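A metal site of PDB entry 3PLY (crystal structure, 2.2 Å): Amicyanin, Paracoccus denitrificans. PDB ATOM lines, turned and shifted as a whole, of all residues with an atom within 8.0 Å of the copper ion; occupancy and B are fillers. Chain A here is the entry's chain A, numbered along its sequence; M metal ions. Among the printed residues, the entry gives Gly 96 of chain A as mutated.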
ATOM      1  N   ILE A  25      -6.517 -10.993  -5.678  1.00  0.00           N
ATOM      2  CA  ILE A  25      -6.894  -9.824  -4.919  1.00  0.00           C
ATOM      3  C   ILE A  25      -8.272 -10.047  -4.359  1.00  0.00           C
ATOM      4  O   ILE A  25      -9.241 -10.166  -5.119  1.00  0.00           O
ATOM      5  CB  ILE A  25      -6.932  -8.611  -5.809  1.00  0.00           C
ATOM      6  CG1 ILE A  25      -5.687  -8.525  -6.688  1.00  0.00           C
ATOM      7  CG2 ILE A  25      -7.065  -7.339  -4.994  1.00  0.00           C
ATOM      8  CD1 ILE A  25      -5.722  -7.281  -7.641  1.00  0.00           C
ATOM      9  N   MET A  28      -9.615  -6.661  -0.139  1.00  0.00           N
ATOM     10  CA  MET A  28      -8.852  -5.414  -0.038  1.00  0.00           C
ATOM     11  C   MET A  28      -7.357  -5.661   0.205  1.00  0.00           C
ATOM     12  O   MET A  28      -6.671  -4.809   0.739  1.00  0.00           O
ATOM     13  CB  MET A  28      -9.421  -4.518   1.071  1.00  0.00           C
ATOM     14  CG  MET A  28     -10.921  -4.255   0.955  1.00  0.00           C
ATOM     15  SD  MET A  28     -11.432  -3.463  -0.597  1.00  0.00           S
ATOM     16  CE  MET A  28     -10.815  -1.799  -0.359  1.00  0.00           C
ATOM     17  N   LYS A  29      -6.886  -6.847  -0.168  1.00  0.00           N
ATOM     18  CA  LYS A  29      -5.461  -7.148  -0.072  1.00  0.00           C
ATOM     19  C   LYS A  29      -4.936  -7.852  -1.319  1.00  0.00           C
ATOM     20  O   LYS A  29      -5.677  -8.582  -1.994  1.00  0.00           O
ATOM     21  CB  LYS A  29      -5.172  -8.069   1.107  1.00  0.00           C
ATOM     22  CG  LYS A  29      -5.580  -7.582   2.480  1.00  0.00           C
ATOM     23  N   TYR A  30      -3.664  -7.633  -1.600  1.00  0.00           N
ATOM     24  CA  TYR A  30      -2.955  -8.486  -2.537  1.00  0.00           C
ATOM     25  C   TYR A  30      -2.611  -9.748  -1.769  1.00  0.00           C
ATOM     26  O   TYR A  30      -1.865  -9.705  -0.796  1.00  0.00           O
ATOM     27  CB  TYR A  30      -1.689  -7.798  -3.030  1.00  0.00           C
ATOM     28  CG  TYR A  30      -1.939  -6.509  -3.782  1.00  0.00           C
ATOM     29  CD1 TYR A  30      -2.540  -6.519  -5.013  1.00  0.00           C
ATOM     30  CD2 TYR A  30      -1.544  -5.283  -3.247  1.00  0.00           C
ATOM     31  CE1 TYR A  30      -2.760  -5.344  -5.707  1.00  0.00           C
ATOM     32  CE2 TYR A  30      -1.765  -4.109  -3.924  1.00  0.00           C
ATOM     33  CZ  TYR A  30      -2.372  -4.139  -5.163  1.00  0.00           C
ATOM     34  OH  TYR A  30      -2.595  -2.956  -5.863  1.00  0.00           O
ATOM     35  N   ASN A  47      -8.552 -10.094  -9.977  1.00  0.00           N
ATOM     36  CA  ASN A  47      -9.418  -9.476  -8.998  1.00  0.00           C
ATOM     37  C   ASN A  47     -10.562 -10.425  -8.698  1.00  0.00           C
ATOM     38  O   ASN A  47     -11.285 -10.803  -9.598  1.00  0.00           O
ATOM     39  CB  ASN A  47      -9.963  -8.145  -9.504  1.00  0.00           C
ATOM     40  CG  ASN A  47     -10.839  -7.457  -8.478  1.00  0.00           C
ATOM     41  OD1 ASN A  47     -10.935  -7.888  -7.328  1.00  0.00           O
ATOM     42  ND2 ASN A  47     -11.497  -6.371  -8.887  1.00  0.00           N
ATOM     43  N   GLU A  49     -12.988  -9.893  -6.400  1.00  0.00           N
ATOM     44  CA  GLU A  49     -14.146  -9.234  -5.815  1.00  0.00           C
ATOM     45  C   GLU A  49     -14.701  -8.094  -6.676  1.00  0.00           C
ATOM     46  O   GLU A  49     -14.191  -7.822  -7.761  1.00  0.00           O
ATOM     47  CB  GLU A  49     -13.857  -8.756  -4.379  1.00  0.00           C
ATOM     48  CG  GLU A  49     -12.674  -7.798  -4.234  1.00  0.00           C
ATOM     49  CD  GLU A  49     -12.400  -7.440  -2.780  1.00  0.00           C
ATOM     50  OE1 GLU A  49     -12.999  -8.090  -1.907  1.00  0.00           O
ATOM     51  OE2 GLU A  49     -11.588  -6.524  -2.522  1.00  0.00           O
ATOM     52  N   MET A  51     -15.225  -4.761  -5.762  1.00  0.00           N
ATOM     53  CA  MET A  51     -14.460  -3.523  -5.655  1.00  0.00           C
ATOM     54  C   MET A  51     -13.327  -3.578  -6.677  1.00  0.00           C
ATOM     55  O   MET A  51     -12.528  -4.503  -6.662  1.00  0.00           O
ATOM     56  CB  MET A  51     -13.892  -3.358  -4.254  1.00  0.00           C
ATOM     57  CG  MET A  51     -12.968  -2.167  -4.104  1.00  0.00           C
ATOM     58  SD  MET A  51     -13.847  -0.590  -4.177  1.00  0.00           S
ATOM     59  CE  MET A  51     -14.648  -0.555  -2.560  1.00  0.00           C
ATOM     60  N   PRO A  52     -13.293  -2.582  -7.596  1.00  0.00           N
ATOM     61  CA  PRO A  52     -12.217  -2.515  -8.603  1.00  0.00           C
ATOM     62  C   PRO A  52     -10.870  -2.285  -7.936  1.00  0.00           C
ATOM     63  O   PRO A  52     -10.803  -1.560  -6.938  1.00  0.00           O
ATOM     64  CB  PRO A  52     -12.601  -1.273  -9.432  1.00  0.00           C
ATOM     65  CG  PRO A  52     -14.059  -1.056  -9.145  1.00  0.00           C
ATOM     66  CD  PRO A  52     -14.236  -1.473  -7.718  1.00  0.00           C
ATOM     67  N   HIS A  53      -9.812  -2.895  -8.466  1.00  0.00           N
ATOM     68  CA  HIS A  53      -8.453  -2.667  -7.977  1.00  0.00           C
ATOM     69  C   HIS A  53      -7.542  -2.652  -9.176  1.00  0.00           C
ATOM     70  O   HIS A  53      -7.921  -3.161 -10.238  1.00  0.00           O
ATOM     71  CB  HIS A  53      -7.961  -3.814  -7.082  1.00  0.00           C
ATOM     72  CG  HIS A  53      -8.800  -4.077  -5.866  1.00  0.00           C
ATOM     73  ND1 HIS A  53      -8.874  -3.205  -4.802  1.00  0.00           N
ATOM     74  CD2 HIS A  53      -9.576  -5.141  -5.527  1.00  0.00           C
ATOM     75  CE1 HIS A  53      -9.653  -3.701  -3.872  1.00  0.00           C
ATOM     76  NE2 HIS A  53     -10.092  -4.889  -4.288  1.00  0.00           N
ATOM     77  N   ASN A  54      -6.352  -2.089  -9.013  1.00  0.00           N
ATOM     78  CA  ASN A  54      -5.322  -2.179 -10.024  1.00  0.00           C
ATOM     79  C   ASN A  54      -3.966  -2.437  -9.376  1.00  0.00           C
ATOM     80  O   ASN A  54      -3.887  -2.668  -8.168  1.00  0.00           O
ATOM     81  CB  ASN A  54      -5.261  -0.910 -10.896  1.00  0.00           C
ATOM     82  CG  ASN A  54      -4.698   0.295 -10.149  1.00  0.00           C
ATOM     83  OD1 ASN A  54      -4.689   0.338  -8.922  1.00  0.00           O
ATOM     84  ND2 ASN A  54      -4.224   1.287 -10.891  1.00  0.00           N
ATOM     85  N   VAL A  55      -2.913  -2.412 -10.172  1.00  0.00           N
ATOM     86  CA  VAL A  55      -1.561  -2.392  -9.633  1.00  0.00           C
ATOM     87  C   VAL A  55      -0.890  -1.186 -10.221  1.00  0.00           C
ATOM     88  O   VAL A  55      -1.091  -0.866 -11.398  1.00  0.00           O
ATOM     89  CB  VAL A  55      -0.771  -3.673  -9.937  1.00  0.00           C
ATOM     90  CG1 VAL A  55      -1.446  -4.888  -9.291  1.00  0.00           C
ATOM     91  CG2 VAL A  55      -0.584  -3.884 -11.451  1.00  0.00           C
ATOM     92  N   MET A  71      -8.007  -0.361 -14.080  1.00  0.00           N
ATOM     93  CA  MET A  71      -8.868  -0.892 -13.042  1.00  0.00           C
ATOM     94  C   MET A  71      -9.453  -2.221 -13.500  1.00  0.00           C
ATOM     95  O   MET A  71      -9.911  -2.350 -14.640  1.00  0.00           O
ATOM     96  CB  MET A  71      -9.981   0.115 -12.715  1.00  0.00           C
ATOM     97  CG  MET A  71      -9.447   1.447 -12.146  1.00  0.00           C
ATOM     98  SD  MET A  71      -8.302   1.223 -10.746  1.00  0.00           S
ATOM     99  CE  MET A  71      -9.427   0.538  -9.531  1.00  0.00           C
ATOM    100  N   MET A  72      -9.410  -3.227 -12.627  1.00  0.00           N
ATOM    101  CA  MET A  72      -9.964  -4.555 -12.889  1.00  0.00           C
ATOM    102  C   MET A  72     -11.257  -4.744 -12.111  1.00  0.00           C
ATOM    103  O   MET A  72     -11.292  -4.586 -10.885  1.00  0.00           O
ATOM    104  CB  MET A  72      -9.004  -5.646 -12.422  1.00  0.00           C
ATOM    105  CG  MET A  72      -7.716  -5.779 -13.200  1.00  0.00           C
ATOM    106  SD  MET A  72      -6.555  -6.855 -12.329  1.00  0.00           S
ATOM    107  CE  MET A  72      -5.702  -5.633 -11.367  1.00  0.00           C
ATOM    108  N   HIS A  91       1.226  -0.467  -5.575  1.00  0.00           N
ATOM    109  CA  HIS A  91       0.074  -0.316  -4.709  1.00  0.00           C
ATOM    110  C   HIS A  91      -1.165  -0.180  -5.569  1.00  0.00           C
ATOM    111  O   HIS A  91      -1.100  -0.156  -6.804  1.00  0.00           O
ATOM    112  CB  HIS A  91       0.231   0.908  -3.803  1.00  0.00           C
ATOM    113  CG  HIS A  91       0.234   2.195  -4.559  1.00  0.00           C
ATOM    114  ND1 HIS A  91       1.345   2.651  -5.249  1.00  0.00           N
ATOM    115  CD2 HIS A  91      -0.735   3.119  -4.765  1.00  0.00           C
ATOM    116  CE1 HIS A  91       1.061   3.802  -5.828  1.00  0.00           C
ATOM    117  NE2 HIS A  91      -0.199   4.104  -5.559  1.00  0.00           N
ATOM    118  N   CYS A  92      -2.310  -0.128  -4.907  1.00  0.00           N
ATOM    119  CA  CYS A  92      -3.541   0.055  -5.603  1.00  0.00           C
ATOM    120  C   CYS A  92      -3.895   1.542  -5.616  1.00  0.00           C
ATOM    121  O   CYS A  92      -3.966   2.192  -4.558  1.00  0.00           O
ATOM    122  CB  CYS A  92      -4.606  -0.759  -4.896  1.00  0.00           C
ATOM    123  SG  CYS A  92      -6.082  -0.668  -5.734  1.00  0.00           S
ATOM    124  N   THR A  93      -4.111   2.102  -6.810  1.00  0.00           N
ATOM    125  CA  THR A  93      -4.231   3.551  -6.951  1.00  0.00           C
ATOM    126  C   THR A  93      -5.267   4.190  -6.029  1.00  0.00           C
ATOM    127  O   THR A  93      -4.942   5.110  -5.291  1.00  0.00           O
ATOM    128  CB  THR A  93      -4.465   3.962  -8.424  1.00  0.00           C
ATOM    129  OG1 THR A  93      -3.353   3.541  -9.222  1.00  0.00           O
ATOM    130  CG2 THR A  93      -4.609   5.507  -8.548  1.00  0.00           C
ATOM    131  N   PRO A  94      -6.515   3.711  -6.091  1.00  0.00           N
ATOM    132  CA  PRO A  94      -7.501   4.234  -5.139  1.00  0.00           C
ATOM    133  C   PRO A  94      -7.346   3.652  -3.725  1.00  0.00           C
ATOM    134  O   PRO A  94      -7.862   4.247  -2.800  1.00  0.00           O
ATOM    135  CB  PRO A  94      -8.835   3.800  -5.758  1.00  0.00           C
ATOM    136  CG  PRO A  94      -8.512   2.584  -6.559  1.00  0.00           C
ATOM    137  CD  PRO A  94      -7.134   2.842  -7.106  1.00  0.00           C
ATOM    138  N   HIS A  95      -6.646   2.528  -3.557  1.00  0.00           N
ATOM    139  CA  HIS A  95      -6.531   1.899  -2.241  1.00  0.00           C
ATOM    140  C   HIS A  95      -5.061   1.820  -1.815  1.00  0.00           C
ATOM    141  O   HIS A  95      -4.451   0.739  -1.812  1.00  0.00           O
ATOM    142  CB  HIS A  95      -7.209   0.507  -2.263  1.00  0.00           C
ATOM    143  CG  HIS A  95      -8.621   0.539  -2.778  1.00  0.00           C
ATOM    144  ND1 HIS A  95      -9.081  -0.313  -3.766  1.00  0.00           N
ATOM    145  CD2 HIS A  95      -9.667   1.335  -2.450  1.00  0.00           C
ATOM    146  CE1 HIS A  95     -10.348  -0.043  -4.021  1.00  0.00           C
ATOM    147  NE2 HIS A  95     -10.729   0.953  -3.233  1.00  0.00           N
ATOM    148  N   GLY A  96      -4.490   2.976  -1.446  1.00  0.00           N
ATOM    149  CA  GLY A  96      -3.067   3.113  -1.209  1.00  0.00           C
ATOM    150  C   GLY A  96      -2.551   2.307  -0.005  1.00  0.00           C
ATOM    151  O   GLY A  96      -1.343   2.141   0.207  1.00  0.00           O
ATOM    152  N   PHE A  97      -3.484   1.812   0.800  1.00  0.00           N
ATOM    153  CA  PHE A  97      -3.114   0.939   1.906  1.00  0.00           C
ATOM    154  C   PHE A  97      -2.838  -0.477   1.409  1.00  0.00           C
ATOM    155  O   PHE A  97      -2.288  -1.296   2.152  1.00  0.00           O
ATOM    156  CB  PHE A  97      -4.219   0.917   2.952  1.00  0.00           C
ATOM    157  CG  PHE A  97      -5.516   0.459   2.423  1.00  0.00           C
ATOM    158  CD1 PHE A  97      -5.832  -0.894   2.374  1.00  0.00           C
ATOM    159  CD2 PHE A  97      -6.436   1.373   1.942  1.00  0.00           C
ATOM    160  CE1 PHE A  97      -7.036  -1.325   1.877  1.00  0.00           C
ATOM    161  CE2 PHE A  97      -7.655   0.945   1.438  1.00  0.00           C
ATOM    162  CZ  PHE A  97      -7.955  -0.411   1.397  1.00  0.00           C
ATOM    163  N   MET A  98      -3.236  -0.768   0.165  1.00  0.00           N
ATOM    164  CA  MET A  98      -2.964  -2.064  -0.445  1.00  0.00           C
ATOM    165  C   MET A  98      -1.619  -1.995  -1.130  1.00  0.00           C
ATOM    166  O   MET A  98      -1.435  -1.283  -2.129  1.00  0.00           O
ATOM    167  CB  MET A  98      -4.009  -2.437  -1.482  1.00  0.00           C
ATOM    168  CG  MET A  98      -5.378  -2.696  -0.939  1.00  0.00           C
ATOM    169  SD  MET A  98      -6.581  -2.918  -2.259  1.00  0.00           S
ATOM    170  CE  MET A  98      -6.004  -4.365  -3.094  1.00  0.00           C
HETATM  171 CU    CU M   1      -7.774  -1.478  -4.747  1.00  0.00          CU
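NE2 of His 95 lies close to SD of Met 51, at 3.6 Å. ND1 of His 53 sits close to SD of Met 98. O of Met 51 lies close to NE2 of His 53, at 3.4 Å. A ring nitrogen (NE2) of His 53 lies within hydrogen-bond range of the side-chain carboxylate (OE2) of Glu 49. The backbone NH (N) of Met 72 sits at hydrogen-bond distance from the backbone carbonyl oxygen (O) of His 53. The backbone NH (N) of Cys 92 sits at hydrogen-bond distance from the backbone carbonyl oxygen (O) of Met 98 (3.1 Å). The backbone NH (N) of Asn 54 sits close to the side-chain sulfur (SG) of Cys 92 (3.6 Å). N of Cys 92 lies within hydrogen-bond range of OH of Tyr 30, at 3.0 Å.
O of Pro 52 touches the copper ion, at 3.7 Å. Met 98 touches the copper ion (SD to CU, 3.1 Å). Along chain A the residues within 4 Å of the copper ion span positions 52 to 98. The nearest printed residue that does not touch the copper ion is Pro 94 (4.5 Å).
The copper ion is bound by ND1 of His 95 (2.0 Å), ND1 of His 53 (2.0 Å) and SG of Cys 92 (2.1 Å). The copper ion has three donor atoms within binding distance.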
